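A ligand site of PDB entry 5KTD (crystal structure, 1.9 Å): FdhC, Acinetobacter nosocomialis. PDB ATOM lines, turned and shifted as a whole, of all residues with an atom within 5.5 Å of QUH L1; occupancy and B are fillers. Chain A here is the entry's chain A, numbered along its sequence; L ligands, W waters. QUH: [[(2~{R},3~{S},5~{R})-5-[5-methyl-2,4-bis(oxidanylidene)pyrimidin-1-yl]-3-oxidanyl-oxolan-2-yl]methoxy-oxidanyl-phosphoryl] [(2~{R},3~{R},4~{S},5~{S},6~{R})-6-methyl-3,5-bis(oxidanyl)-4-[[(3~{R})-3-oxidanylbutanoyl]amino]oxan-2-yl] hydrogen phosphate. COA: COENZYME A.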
ATOM      1  N   ILE A  24     -29.719 -31.097   2.694  1.00  0.00           N
ATOM      2  CA  ILE A  24     -28.572 -30.532   1.964  1.00  0.00           C
ATOM      3  C   ILE A  24     -29.009 -29.884   0.656  1.00  0.00           C
ATOM      4  O   ILE A  24     -28.558 -28.761   0.375  1.00  0.00           O
ATOM      5  CB  ILE A  24     -27.452 -31.557   1.757  1.00  0.00           C
ATOM      6  CG1 ILE A  24     -26.860 -31.950   3.124  1.00  0.00           C
ATOM      7  CG2 ILE A  24     -26.320 -30.938   0.956  1.00  0.00           C
ATOM      8  CD1 ILE A  24     -25.881 -33.097   3.095  1.00  0.00           C
ATOM      9  N   ARG A  28     -28.369 -25.917  -0.002  1.00  0.00           N
ATOM     10  CA  ARG A  28     -27.406 -25.519  -1.038  1.00  0.00           C
ATOM     11  C   ARG A  28     -28.083 -24.853  -2.224  1.00  0.00           C
ATOM     12  O   ARG A  28     -27.424 -24.138  -2.942  1.00  0.00           O
ATOM     13  CB  ARG A  28     -26.613 -26.710  -1.514  1.00  0.00           C
ATOM     14  CG  ARG A  28     -25.646 -27.232  -0.440  1.00  0.00           C
ATOM     15  CD  ARG A  28     -24.755 -28.306  -0.994  1.00  0.00           C
ATOM     16  NE  ARG A  28     -23.828 -27.741  -1.970  1.00  0.00           N
ATOM     17  CZ  ARG A  28     -22.584 -27.334  -1.757  1.00  0.00           C
ATOM     18  NH1 ARG A  28     -22.023 -27.422  -0.539  1.00  0.00           N
ATOM     19  NH2 ARG A  28     -21.884 -26.790  -2.758  1.00  0.00           N
ATOM     20  N   TYR A  36     -21.844 -17.586  -2.758  1.00  0.00           N
ATOM     21  CA  TYR A  36     -20.414 -17.743  -2.799  1.00  0.00           C
ATOM     22  C   TYR A  36     -19.958 -19.213  -2.668  1.00  0.00           C
ATOM     23  O   TYR A  36     -18.799 -19.447  -2.323  1.00  0.00           O
ATOM     24  CB  TYR A  36     -19.805 -16.875  -1.682  1.00  0.00           C
ATOM     25  CG  TYR A  36     -20.111 -15.410  -1.860  1.00  0.00           C
ATOM     26  CD1 TYR A  36     -19.571 -14.679  -2.918  1.00  0.00           C
ATOM     27  CD2 TYR A  36     -20.940 -14.746  -0.970  1.00  0.00           C
ATOM     28  CE1 TYR A  36     -19.842 -13.347  -3.085  1.00  0.00           C
ATOM     29  CE2 TYR A  36     -21.229 -13.406  -1.117  1.00  0.00           C
ATOM     30  CZ  TYR A  36     -20.690 -12.700  -2.176  1.00  0.00           C
ATOM     31  OH  TYR A  36     -20.954 -11.355  -2.295  1.00  0.00           O
ATOM     32  N   ILE A  37     -20.832 -20.188  -2.937  1.00  0.00           N
ATOM     33  CA  ILE A  37     -20.411 -21.597  -2.837  1.00  0.00           C
ATOM     34  C   ILE A  37     -20.633 -22.221  -4.188  1.00  0.00           C
ATOM     35  O   ILE A  37     -21.204 -21.579  -5.042  1.00  0.00           O
ATOM     36  CB  ILE A  37     -21.141 -22.350  -1.717  1.00  0.00           C
ATOM     37  CG1 ILE A  37     -22.621 -22.524  -2.037  1.00  0.00           C
ATOM     38  CG2 ILE A  37     -20.953 -21.578  -0.412  1.00  0.00           C
ATOM     39  CD1 ILE A  37     -23.424 -23.262  -0.992  1.00  0.00           C
ATOM     40  N   SER A  38     -20.204 -23.477  -4.366  1.00  0.00           N
ATOM     41  CA  SER A  38     -20.363 -24.170  -5.640  1.00  0.00           C
ATOM     42  C   SER A  38     -21.815 -24.517  -5.882  1.00  0.00           C
ATOM     43  O   SER A  38     -22.504 -24.931  -4.950  1.00  0.00           O
ATOM     44  CB  SER A  38     -19.568 -25.490  -5.706  1.00  0.00           C
ATOM     45  OG  SER A  38     -18.181 -25.268  -5.602  1.00  0.00           O
ATOM     46  N   LYS A  39     -22.265 -24.333  -7.131  1.00  0.00           N
ATOM     47  CA  LYS A  39     -23.504 -24.922  -7.632  1.00  0.00           C
ATOM     48  C   LYS A  39     -23.561 -26.409  -7.342  1.00  0.00           C
ATOM     49  O   LYS A  39     -22.568 -27.140  -7.496  1.00  0.00           O
ATOM     50  CB  LYS A  39     -23.580 -24.820  -9.154  1.00  0.00           C
ATOM     51  CG  LYS A  39     -23.856 -23.447  -9.701  1.00  0.00           C
ATOM     52  CD  LYS A  39     -23.999 -23.514 -11.224  1.00  0.00           C
ATOM     53  CE  LYS A  39     -24.365 -22.155 -11.791  1.00  0.00           C
ATOM     54  NZ  LYS A  39     -24.529 -22.120 -13.283  1.00  0.00           N
ATOM     55  N   SER A  40     -24.744 -26.868  -6.945  1.00  0.00           N
ATOM     56  CA  SER A  40     -24.941 -28.294  -6.743  1.00  0.00           C
ATOM     57  C   SER A  40     -26.375 -28.727  -6.987  1.00  0.00           C
ATOM     58  O   SER A  40     -27.299 -27.910  -6.970  1.00  0.00           O
ATOM     59  CB  SER A  40     -24.464 -28.704  -5.331  1.00  0.00           C
ATOM     60  OG  SER A  40     -25.258 -28.199  -4.267  1.00  0.00           O
ATOM     61  N   THR A  41     -26.545 -30.011  -7.242  1.00  0.00           N
ATOM     62  CA  THR A  41     -27.813 -30.533  -7.669  1.00  0.00           C
ATOM     63  C   THR A  41     -28.928 -30.217  -6.682  1.00  0.00           C
ATOM     64  O   THR A  41     -28.741 -30.248  -5.437  1.00  0.00           O
ATOM     65  CB  THR A  41     -27.772 -32.058  -7.891  1.00  0.00           C
ATOM     66  OG1 THR A  41     -29.082 -32.447  -8.230  1.00  0.00           O
ATOM     67  CG2 THR A  41     -27.386 -32.867  -6.593  1.00  0.00           C
ATOM     68  N   GLN A  47     -28.113 -35.962  -4.861  1.00  0.00           N
ATOM     69  CA  GLN A  47     -27.390 -35.596  -3.644  1.00  0.00           C
ATOM     70  C   GLN A  47     -27.128 -36.872  -2.832  1.00  0.00           C
ATOM     71  O   GLN A  47     -26.058 -37.012  -2.338  1.00  0.00           O
ATOM     72  CB  GLN A  47     -28.134 -34.520  -2.885  1.00  0.00           C
ATOM     73  CG  GLN A  47     -27.501 -34.093  -1.573  1.00  0.00           C
ATOM     74  CD  GLN A  47     -26.140 -33.488  -1.719  1.00  0.00           C
ATOM     75  OE1 GLN A  47     -25.889 -32.715  -2.610  1.00  0.00           O
ATOM     76  NE2 GLN A  47     -25.263 -33.798  -0.778  1.00  0.00           N
ATOM     77  N   TRP A  50     -24.077 -38.425  -4.241  1.00  0.00           N
ATOM     78  CA  TRP A  50     -22.893 -37.676  -3.788  1.00  0.00           C
ATOM     79  C   TRP A  50     -22.474 -38.131  -2.387  1.00  0.00           C
ATOM     80  O   TRP A  50     -21.270 -38.344  -2.098  1.00  0.00           O
ATOM     81  CB  TRP A  50     -23.197 -36.149  -3.817  1.00  0.00           C
ATOM     82  CG  TRP A  50     -21.980 -35.293  -3.775  1.00  0.00           C
ATOM     83  CD1 TRP A  50     -21.372 -34.663  -4.845  1.00  0.00           C
ATOM     84  CD2 TRP A  50     -21.205 -34.966  -2.633  1.00  0.00           C
ATOM     85  NE1 TRP A  50     -20.259 -33.974  -4.417  1.00  0.00           N
ATOM     86  CE2 TRP A  50     -20.146 -34.143  -3.068  1.00  0.00           C
ATOM     87  CE3 TRP A  50     -21.295 -35.293  -1.276  1.00  0.00           C
ATOM     88  CZ2 TRP A  50     -19.180 -33.656  -2.181  1.00  0.00           C
ATOM     89  CZ3 TRP A  50     -20.317 -34.777  -0.410  1.00  0.00           C
ATOM     90  CH2 TRP A  50     -19.285 -34.000  -0.868  1.00  0.00           C
ATOM     91  N   TYR A  65     -17.803 -35.100   6.822  1.00  0.00           N
ATOM     92  CA  TYR A  65     -18.844 -34.181   6.422  1.00  0.00           C
ATOM     93  C   TYR A  65     -19.886 -34.246   7.497  1.00  0.00           C
ATOM     94  O   TYR A  65     -20.299 -35.339   7.873  1.00  0.00           O
ATOM     95  CB  TYR A  65     -19.393 -34.652   5.110  1.00  0.00           C
ATOM     96  CG  TYR A  65     -20.312 -33.732   4.342  1.00  0.00           C
ATOM     97  CD1 TYR A  65     -20.441 -32.391   4.648  1.00  0.00           C
ATOM     98  CD2 TYR A  65     -21.030 -34.211   3.237  1.00  0.00           C
ATOM     99  CE1 TYR A  65     -21.263 -31.556   3.868  1.00  0.00           C
ATOM    100  CE2 TYR A  65     -21.867 -33.390   2.507  1.00  0.00           C
ATOM    101  CZ  TYR A  65     -21.995 -32.064   2.847  1.00  0.00           C
ATOM    102  OH  TYR A  65     -22.827 -31.201   2.097  1.00  0.00           O
ATOM    103  N   ARG A  81     -17.641 -29.257   6.423  1.00  0.00           N
ATOM    104  CA  ARG A  81     -16.852 -30.383   5.862  1.00  0.00           C
ATOM    105  C   ARG A  81     -15.346 -30.201   6.011  1.00  0.00           C
ATOM    106  O   ARG A  81     -14.843 -29.107   5.754  1.00  0.00           O
ATOM    107  CB  ARG A  81     -17.200 -30.544   4.379  1.00  0.00           C
ATOM    108  CG  ARG A  81     -16.707 -31.822   3.729  1.00  0.00           C
ATOM    109  CD  ARG A  81     -17.436 -32.092   2.404  1.00  0.00           C
ATOM    110  NE  ARG A  81     -17.168 -30.987   1.479  1.00  0.00           N
ATOM    111  CZ  ARG A  81     -16.443 -31.005   0.340  1.00  0.00           C
ATOM    112  NH1 ARG A  81     -15.913 -32.109  -0.155  1.00  0.00           N
ATOM    113  NH2 ARG A  81     -16.309 -29.865  -0.347  1.00  0.00           N
ATOM    114  N   TYR A  83     -11.871 -31.902   4.450  1.00  0.00           N
ATOM    115  CA  TYR A  83     -11.550 -32.628   3.209  1.00  0.00           C
ATOM    116  C   TYR A  83     -10.160 -32.235   2.654  1.00  0.00           C
ATOM    117  O   TYR A  83      -9.526 -31.288   3.118  1.00  0.00           O
ATOM    118  CB  TYR A  83     -12.675 -32.399   2.172  1.00  0.00           C
ATOM    119  CG  TYR A  83     -12.791 -30.961   1.636  1.00  0.00           C
ATOM    120  CD1 TYR A  83     -13.194 -29.901   2.459  1.00  0.00           C
ATOM    121  CD2 TYR A  83     -12.475 -30.647   0.249  1.00  0.00           C
ATOM    122  CE1 TYR A  83     -13.279 -28.596   1.950  1.00  0.00           C
ATOM    123  CE2 TYR A  83     -12.543 -29.349  -0.233  1.00  0.00           C
ATOM    124  CZ  TYR A  83     -12.930 -28.312   0.620  1.00  0.00           C
ATOM    125  OH  TYR A  83     -13.063 -26.999   0.146  1.00  0.00           O
ATOM    126  N   TRP A  94     -11.050 -27.239   5.063  1.00  0.00           N
ATOM    127  CA  TRP A  94     -12.430 -27.235   5.468  1.00  0.00           C
ATOM    128  C   TRP A  94     -13.252 -26.193   4.716  1.00  0.00           C
ATOM    129  O   TRP A  94     -12.716 -25.292   4.075  1.00  0.00           O
ATOM    130  CB  TRP A  94     -12.580 -27.104   6.966  1.00  0.00           C
ATOM    131  CG  TRP A  94     -12.386 -25.747   7.603  1.00  0.00           C
ATOM    132  CD1 TRP A  94     -11.211 -25.134   7.920  1.00  0.00           C
ATOM    133  CD2 TRP A  94     -13.427 -24.933   8.151  1.00  0.00           C
ATOM    134  NE1 TRP A  94     -11.467 -23.948   8.625  1.00  0.00           N
ATOM    135  CE2 TRP A  94     -12.817 -23.826   8.783  1.00  0.00           C
ATOM    136  CE3 TRP A  94     -14.827 -25.038   8.174  1.00  0.00           C
ATOM    137  CZ2 TRP A  94     -13.558 -22.792   9.418  1.00  0.00           C
ATOM    138  CZ3 TRP A  94     -15.578 -23.979   8.790  1.00  0.00           C
ATOM    139  CH2 TRP A  94     -14.926 -22.899   9.428  1.00  0.00           C
ATOM    140  N   GLY A  95     -14.549 -26.372   4.792  1.00  0.00           N
ATOM    141  CA  GLY A  95     -15.492 -25.557   4.045  1.00  0.00           C
ATOM    142  C   GLY A  95     -16.821 -26.235   3.912  1.00  0.00           C
ATOM    143  O   GLY A  95     -17.264 -26.880   4.884  1.00  0.00           O
ATOM    144  N   SER A  96     -17.495 -26.059   2.768  1.00  0.00           N
ATOM    145  CA  SER A  96     -18.911 -26.431   2.659  1.00  0.00           C
ATOM    146  C   SER A  96     -19.715 -25.887   3.852  1.00  0.00           C
ATOM    147  O   SER A  96     -20.618 -26.543   4.359  1.00  0.00           O
ATOM    148  CB  SER A  96     -19.097 -27.957   2.518  1.00  0.00           C
ATOM    149  OG  SER A  96     -18.351 -28.471   1.429  1.00  0.00           O
ATOM    150  N   TRP A  97     -19.405 -24.663   4.243  1.00  0.00           N
ATOM    151  CA  TRP A  97     -19.802 -24.124   5.540  1.00  0.00           C
ATOM    152  C   TRP A  97     -21.015 -23.199   5.330  1.00  0.00           C
ATOM    153  O   TRP A  97     -20.888 -22.114   4.762  1.00  0.00           O
ATOM    154  CB  TRP A  97     -18.661 -23.360   6.134  1.00  0.00           C
ATOM    155  CG  TRP A  97     -18.853 -22.928   7.551  1.00  0.00           C
ATOM    156  CD1 TRP A  97     -19.464 -23.608   8.571  1.00  0.00           C
ATOM    157  CD2 TRP A  97     -18.335 -21.734   8.114  1.00  0.00           C
ATOM    158  NE1 TRP A  97     -19.392 -22.860   9.734  1.00  0.00           N
ATOM    159  CE2 TRP A  97     -18.680 -21.730   9.482  1.00  0.00           C
ATOM    160  CE3 TRP A  97     -17.597 -20.648   7.577  1.00  0.00           C
ATOM    161  CZ2 TRP A  97     -18.343 -20.691  10.325  1.00  0.00           C
ATOM    162  CZ3 TRP A  97     -17.259 -19.601   8.427  1.00  0.00           C
ATOM    163  CH2 TRP A  97     -17.649 -19.635   9.792  1.00  0.00           C
ATOM    164  N   PHE A 130      -8.040 -23.158   3.668  1.00  0.00           N
ATOM    165  CA  PHE A 130      -9.338 -22.898   3.115  1.00  0.00           C
ATOM    166  C   PHE A 130      -9.299 -21.596   2.310  1.00  0.00           C
ATOM    167  O   PHE A 130      -8.354 -20.820   2.417  1.00  0.00           O
ATOM    168  CB  PHE A 130     -10.427 -22.811   4.219  1.00  0.00           C
ATOM    169  CG  PHE A 130     -10.160 -21.778   5.245  1.00  0.00           C
ATOM    170  CD1 PHE A 130      -9.443 -22.091   6.389  1.00  0.00           C
ATOM    171  CD2 PHE A 130     -10.610 -20.481   5.059  1.00  0.00           C
ATOM    172  CE1 PHE A 130      -9.228 -21.118   7.356  1.00  0.00           C
ATOM    173  CE2 PHE A 130     -10.382 -19.501   6.035  1.00  0.00           C
ATOM    174  CZ  PHE A 130      -9.706 -19.828   7.161  1.00  0.00           C
ATOM    175  N   GLU A 131     -10.354 -21.354   1.572  1.00  0.00           N
ATOM    176  CA  GLU A 131     -10.474 -20.171   0.778  1.00  0.00           C
ATOM    177  C   GLU A 131     -11.869 -19.622   0.873  1.00  0.00           C
ATOM    178  O   GLU A 131     -12.776 -20.339   1.248  1.00  0.00           O
ATOM    179  CB  GLU A 131     -10.109 -20.470  -0.683  1.00  0.00           C
ATOM    180  CG  GLU A 131     -11.028 -21.374  -1.470  1.00  0.00           C
ATOM    181  CD  GLU A 131     -10.579 -22.805  -1.519  1.00  0.00           C
ATOM    182  OE1 GLU A 131     -11.412 -23.706  -1.603  1.00  0.00           O
ATOM    183  OE2 GLU A 131      -9.390 -23.051  -1.515  1.00  0.00           O
ATOM    184  N   VAL A 132     -12.020 -18.362   0.498  1.00  0.00           N
ATOM    185  CA  VAL A 132     -13.265 -17.641   0.612  1.00  0.00           C
ATOM    186  C   VAL A 132     -13.327 -16.754  -0.614  1.00  0.00           C
ATOM    187  O   VAL A 132     -12.332 -16.101  -0.932  1.00  0.00           O
ATOM    188  CB  VAL A 132     -13.228 -16.727   1.836  1.00  0.00           C
ATOM    189  CG1 VAL A 132     -14.488 -15.870   1.954  1.00  0.00           C
ATOM    190  CG2 VAL A 132     -12.942 -17.547   3.124  1.00  0.00           C
ATOM    191  N   MET A 133     -14.462 -16.748  -1.299  1.00  0.00           N
ATOM    192  CA  MET A 133     -14.627 -15.863  -2.466  1.00  0.00           C
ATOM    193  C   MET A 133     -14.438 -14.409  -2.181  1.00  0.00           C
ATOM    194  O   MET A 133     -14.945 -13.905  -1.208  1.00  0.00           O
ATOM    195  CB  MET A 133     -15.989 -16.027  -3.130  1.00  0.00           C
ATOM    196  CG  MET A 133     -16.058 -17.341  -3.909  1.00  0.00           C
ATOM    197  SD  MET A 133     -17.397 -17.432  -5.122  1.00  0.00           S
ATOM    198  CE  MET A 133     -16.776 -16.293  -6.371  1.00  0.00           C
ATOM    199  N   VAL A 139     -17.177 -13.058   5.719  1.00  0.00           N
ATOM    200  CA  VAL A 139     -16.514 -14.371   5.961  1.00  0.00           C
ATOM    201  C   VAL A 139     -14.989 -14.141   6.098  1.00  0.00           C
ATOM    202  O   VAL A 139     -14.323 -14.629   7.039  1.00  0.00           O
ATOM    203  CB  VAL A 139     -16.943 -15.393   4.875  1.00  0.00           C
ATOM    204  CG1 VAL A 139     -16.247 -16.755   5.067  1.00  0.00           C
ATOM    205  CG2 VAL A 139     -18.470 -15.547   4.917  1.00  0.00           C
ATOM    206  N   HIS A 143     -12.786 -14.942   9.568  1.00  0.00           N
ATOM    207  CA  HIS A 143     -11.561 -15.778   9.633  1.00  0.00           C
ATOM    208  C   HIS A 143     -10.381 -14.966  10.135  1.00  0.00           C
ATOM    209  O   HIS A 143      -9.611 -15.469  10.957  1.00  0.00           O
ATOM    210  CB  HIS A 143     -11.235 -16.458   8.283  1.00  0.00           C
ATOM    211  CG  HIS A 143     -12.241 -17.489   7.880  1.00  0.00           C
ATOM    212  ND1 HIS A 143     -12.523 -18.581   8.657  1.00  0.00           N
ATOM    213  CD2 HIS A 143     -13.063 -17.559   6.813  1.00  0.00           C
ATOM    214  CE1 HIS A 143     -13.467 -19.294   8.061  1.00  0.00           C
ATOM    215  NE2 HIS A 143     -13.806 -18.693   6.937  1.00  0.00           N
HETATM  216  O1  QUH L   1     -16.657 -22.908   2.946  1.00  0.00           O
HETATM  217  C1  QUH L   1     -15.493 -22.615   2.614  1.00  0.00           C
HETATM  218  C2  QUH L   1     -14.401 -22.260   3.567  1.00  0.00           C
HETATM  219  C3  QUH L   1     -14.935 -21.845   4.913  1.00  0.00           C
HETATM  220  O2  QUH L   1     -15.188 -20.434   4.939  1.00  0.00           O
HETATM  221  C4  QUH L   1     -13.967 -22.087   6.035  1.00  0.00           C
HETATM  222  N1  QUH L   1     -15.082 -22.600   1.292  1.00  0.00           N
HETATM  223  C5  QUH L   1     -15.900 -23.153   0.209  1.00  0.00           C
HETATM  224  C6  QUH L   1     -15.811 -22.260  -1.028  1.00  0.00           C
HETATM  225  O3  QUH L   1     -16.236 -20.925  -0.658  1.00  0.00           O
HETATM  226  C7  QUH L   1     -16.734 -22.858  -2.095  1.00  0.00           C
HETATM  227  C8  QUH L   1     -16.784 -22.037  -3.381  1.00  0.00           C
HETATM  228  O4  QUH L   1     -16.303 -24.196  -2.411  1.00  0.00           O
HETATM  229  C9  QUH L   1     -15.380 -24.498  -0.222  1.00  0.00           C
HETATM  230  O5  QUH L   1     -15.266 -25.412   0.847  1.00  0.00           O
HETATM  231  C10 QUH L   1     -16.223 -25.087  -1.294  1.00  0.00           C
HETATM  232  O6  QUH L   1     -17.506 -25.378  -0.747  1.00  0.00           O
HETATM  233  P1  QUH L   1     -18.466 -26.326  -1.513  1.00  0.00           P
HETATM  234  O7  QUH L   1     -19.227 -25.646  -2.659  1.00  0.00           O
HETATM  235  O8  QUH L   1     -19.368 -26.920  -0.383  1.00  0.00           O
HETATM  236  O9  QUH L   1     -17.807 -27.712  -1.978  1.00  0.00           O
HETATM  237  P2  QUH L   1     -16.877 -28.020  -3.251  1.00  0.00           P
HETATM  238  O10 QUH L   1     -15.612 -28.636  -2.896  1.00  0.00           O
HETATM  239  O11 QUH L   1     -16.668 -26.776  -4.114  1.00  0.00           O
HETATM  240  O12 QUH L   1     -17.713 -29.126  -4.000  1.00  0.00           O
HETATM  241  C11 QUH L   1     -17.188 -30.033  -4.961  1.00  0.00           C
HETATM  242  C12 QUH L   1     -18.350 -30.366  -5.865  1.00  0.00           C
HETATM  243  C13 QUH L   1     -19.107 -29.116  -6.358  1.00  0.00           C
HETATM  244  O13 QUH L   1     -19.597 -29.352  -7.691  1.00  0.00           O
HETATM  245  C14 QUH L   1     -20.361 -29.025  -5.484  1.00  0.00           C
HETATM  246  C15 QUH L   1     -20.630 -30.492  -5.202  1.00  0.00           C
HETATM  247  O14 QUH L   1     -19.337 -31.169  -5.190  1.00  0.00           O
HETATM  248  N2  QUH L   1     -21.271 -30.816  -3.943  1.00  0.00           N
HETATM  249  C16 QUH L   1     -20.620 -30.550  -2.764  1.00  0.00           C
HETATM  250  C17 QUH L   1     -21.194 -30.920  -1.537  1.00  0.00           C
HETATM  251  C18 QUH L   1     -20.510 -30.681  -0.209  1.00  0.00           C
HETATM  252  C19 QUH L   1     -22.494 -31.526  -1.598  1.00  0.00           C
HETATM  253  O15 QUH L   1     -23.089 -31.895  -0.521  1.00  0.00           O
HETATM  254  N3  QUH L   1     -23.097 -31.766  -2.756  1.00  0.00           N
HETATM  255  C20 QUH L   1     -22.509 -31.434  -3.901  1.00  0.00           C
HETATM  256  O16 QUH L   1     -23.189 -31.719  -4.991  1.00  0.00           O
HETATM  257  N1A COA L   2     -15.531 -13.531  18.419  1.00  0.00           N
HETATM  258  C2A COA L   2     -16.706 -13.134  18.939  1.00  0.00           C
HETATM  259  N3A COA L   2     -17.819 -13.070  18.230  1.00  0.00           N
HETATM  260  C4A COA L   2     -17.834 -13.422  16.936  1.00  0.00           C
HETATM  261  C5A COA L   2     -16.601 -13.872  16.294  1.00  0.00           C
HETATM  262  C6A COA L   2     -15.412 -13.893  17.134  1.00  0.00           C
HETATM  263  N6A COA L   2     -14.236 -14.304  16.649  1.00  0.00           N
HETATM  264  N7A COA L   2     -16.874 -14.179  15.021  1.00  0.00           N
HETATM  265  C8A COA L   2     -18.187 -13.914  14.852  1.00  0.00           C
HETATM  266  N9A COA L   2     -18.759 -13.437  16.002  1.00  0.00           N
HETATM  267  C1B COA L   2     -20.191 -13.079  16.175  1.00  0.00           C
HETATM  268  C2B COA L   2     -20.706 -12.203  15.042  1.00  0.00           C
HETATM  269  O2B COA L   2     -20.571 -10.781  15.199  1.00  0.00           O
HETATM  270  C3B COA L   2     -22.146 -12.634  14.926  1.00  0.00           C
HETATM  271  O3B COA L   2     -22.934 -11.924  15.889  1.00  0.00           O
HETATM  272  P3B COA L   2     -23.797 -10.658  15.351  1.00  0.00           P
HETATM  273  O7A COA L   2     -25.147 -11.290  14.995  1.00  0.00           O
HETATM  274  O8A COA L   2     -23.868  -9.843  16.630  1.00  0.00           O
HETATM  275  O9A COA L   2     -23.021 -10.024  14.209  1.00  0.00           O
HETATM  276  C4B COA L   2     -22.120 -14.102  15.248  1.00  0.00           C
HETATM  277  O4B COA L   2     -20.934 -14.300  16.038  1.00  0.00           O
HETATM  278  C5B COA L   2     -22.172 -14.994  13.994  1.00  0.00           C
HETATM  279  O5B COA L   2     -21.047 -14.745  13.145  1.00  0.00           O
HETATM  280  P1A COA L   2     -21.269 -14.272  11.641  1.00  0.00           P
HETATM  281  O1A COA L   2     -19.968 -13.764  11.142  1.00  0.00           O
HETATM  282  O2A COA L   2     -22.505 -13.456  11.358  1.00  0.00           O
HETATM  283  O3A COA L   2     -21.489 -15.669  10.875  1.00  0.00           O
HETATM  284  P2A COA L   2     -22.776 -16.141  10.074  1.00  0.00           P
HETATM  285  O4A COA L   2     -23.921 -16.501  11.013  1.00  0.00           O
HETATM  286  O5A COA L   2     -23.058 -15.389   8.825  1.00  0.00           O
HETATM  287  O6A COA L   2     -22.248 -17.565   9.517  1.00  0.00           O
HETATM  288  CBP COA L   2     -21.620 -18.442   7.386  1.00  0.00           C
HETATM  289  CCP COA L   2     -21.208 -17.538   8.539  1.00  0.00           C
HETATM  290  CDP COA L   2     -20.510 -18.350   6.347  1.00  0.00           C
HETATM  291  CEP COA L   2     -21.773 -19.849   7.958  1.00  0.00           C
HETATM  292  CAP COA L   2     -22.965 -17.969   6.801  1.00  0.00           C
HETATM  293  OAP COA L   2     -22.926 -16.544   6.604  1.00  0.00           O
HETATM  294  C9P COA L   2     -23.367 -18.689   5.558  1.00  0.00           C
HETATM  295  O9P COA L   2     -23.979 -19.743   5.607  1.00  0.00           O
HETATM  296  N8P COA L   2     -23.042 -18.078   4.409  1.00  0.00           N
HETATM  297  C7P COA L   2     -23.438 -18.551   3.126  1.00  0.00           C
HETATM  298  C6P COA L   2     -22.600 -19.736   2.646  1.00  0.00           C
HETATM  299  C5P COA L   2     -21.143 -19.334   2.541  1.00  0.00           C
HETATM  300  O5P COA L   2     -20.831 -18.316   1.911  1.00  0.00           O
HETATM  301  N4P COA L   2     -20.259 -20.103   3.175  1.00  0.00           N
HETATM  302  C3P COA L   2     -18.837 -19.783   3.271  1.00  0.00           C
HETATM  303  C2P COA L   2     -18.020 -20.069   1.993  1.00  0.00           C
HETATM  304  S1P COA L   2     -16.361 -19.335   2.145  1.00  0.00           S
HETATM  305  O   HOH W   1     -16.920 -17.996  -0.629  1.00  0.00           O
HETATM  306  O   HOH W   2     -20.491 -26.738  -9.212  1.00  0.00           O
HETATM  307  O   HOH W   3     -14.127 -20.003  -2.486  1.00  0.00           O
HETATM  308  O   HOH W   4     -12.170 -23.815   1.245  1.00  0.00           O
HETATM  309  O   HOH W   5     -13.421 -27.135  -2.332  1.00  0.00           O
HETATM  310  O   HOH W   6     -24.120 -31.485  -7.436  1.00  0.00           O
HETATM  311  O   HOH W   7     -14.243 -25.312  -4.201  1.00  0.00           O
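Water W6 bridges an oxygen (O16) of QUH L1 and the backbone NH of Thr 41.
Water W5 lies within hydrogen-bond range of the side-chain hydroxyl (OH) of Tyr 83 (2.5 Å) and an oxygen (O10) of QUH L1 (2.7 Å).
Water W3 lies within hydrogen-bond range of O3 of QUH L1 and N of Met 133.
Water W1 lies within hydrogen-bond range of N of Met 133 (2.8 Å), O of Tyr 36 (2.9 Å), O3 of QUH L1 (3.0 Å) and S1P of COA L2 (3.1 Å).
Water W2 bridges the backbone carbonyl oxygen (O) of Lys 39 (2.7 Å) and an oxygen (O13) of QUH L1 (3.2 Å).
Water W4 lies within hydrogen-bond range of OE1 of Glu 131, N1 of QUH L1, O of Trp 94 and OH of Tyr 83.
The side-chain hydroxyl of Ser 96 lies within hydrogen-bond range of an oxygen (O8) of QUH L1 (2.6 Å).
The side-chain hydroxyl (OH) of Tyr 65 lies within hydrogen-bond range of an oxygen (O15) of QUH L1 (2.7 Å).
The backbone carbonyl oxygen (O) of Glu 131 sits at hydrogen-bond distance from a nitrogen (N1) of QUH L1 (3.2 Å).
The side-chain hydroxyl of Tyr 83 sits at hydrogen-bond distance from an oxygen (O5) of QUH L1, at 2.8 Å.
The guanidinium group (NH2) of Arg 81 is in salt-bridge range of an oxygen (O10) of QUH L1 (2.9 Å).
An oxygen (O11) of QUH L1 sits at hydrogen-bond distance from the side-chain hydroxyl (OG) of Ser 38 (2.6 Å).
NE2 of Gln 47 is in hydrogen-bond range of O15 of QUH L1.
O5 of QUH L1 sits at hydrogen-bond distance from N of Ser 96 (3.0 Å).
The indole nitrogen (NE1) of Trp 50 is in hydrogen-bond range of an oxygen (O14) of QUH L1 (3.1 Å).
The guanidinium group (NH1) of Arg 28 lies within salt-bridge range of an oxygen (O8) of QUH L1, at 2.7 Å.
The backbone carbonyl oxygen (O) of Trp 97 lies within hydrogen-bond range of a nitrogen (N4P) of COA L2 (2.6 Å).
An oxygen (O3) of QUH L1 is in hydrogen-bond range of the backbone carbonyl oxygen of Tyr 36 (3.4 Å).
An oxygen (O7) of QUH L1 lies within hydrogen-bond range of the backbone NH (N) of Ser 38, 2.9 Å away.
A ring nitrogen (NE2) of His 143 sits at hydrogen-bond distance from an oxygen (O2) of QUH L1, at 3.0 Å.
O of Gly 95 is in hydrogen-bond range of N of Arg 81, at 2.9 Å.
The guanidinium group (NE) of Arg 81 lies within hydrogen-bond range of the side-chain hydroxyl (OG) of Ser 96 (2.8 Å).
The side-chain hydroxyl (OG) of Ser 40 is in hydrogen-bond range of the guanidinium group (NE) of Arg 28 (2.7 Å).
The backbone carbonyl oxygen (O) of Ser 38 is in hydrogen-bond range of the guanidinium group (NH2) of Arg 28 (2.9 Å).
CG2 of Ile 24 touches O15 of QUH L1 (3.7 Å).
Ile 37 touches QUH L1.
O of Lys 39 touches C14 of QUH L1 (3.5 Å).
CB of Ser 40 touches O16 of QUH L1, 3.3 Å away.
CE2 of Trp 94 touches C4 of QUH L1, at 3.4 Å.
CA of Gly 95 touches O1 of QUH L1 (3.1 Å).
Trp 97 touches QUH L1 (N to O1, 3.5 Å).
Phe 130 touches QUH L1 (CD2 to C4, 3.8 Å).
Val 139 touches QUH L1 (CG1 to O2, 3.8 Å).
Hydrophobic or aromatic side chains within 4 Å of QUH L1: Ile 24, Ile 37, Trp 50, Tyr 65, Tyr 83, Trp 94, Trp 97, Phe 130, Val 139 and His 143.
20 residues have an atom within 4 Å of QUH L1: Ile 24, Arg 28, Tyr 36, Ile 37, Ser 38, Lys 39, Ser 40, Gln 47, Trp 50, Tyr 65, Arg 81, Tyr 83, Trp 94, Gly 95, Ser 96, Trp 97, Phe 130, Glu 131, Val 139 and His 143.
O2 of QUH L1 sits close to S1P of COA L2, at 3.2 Å.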
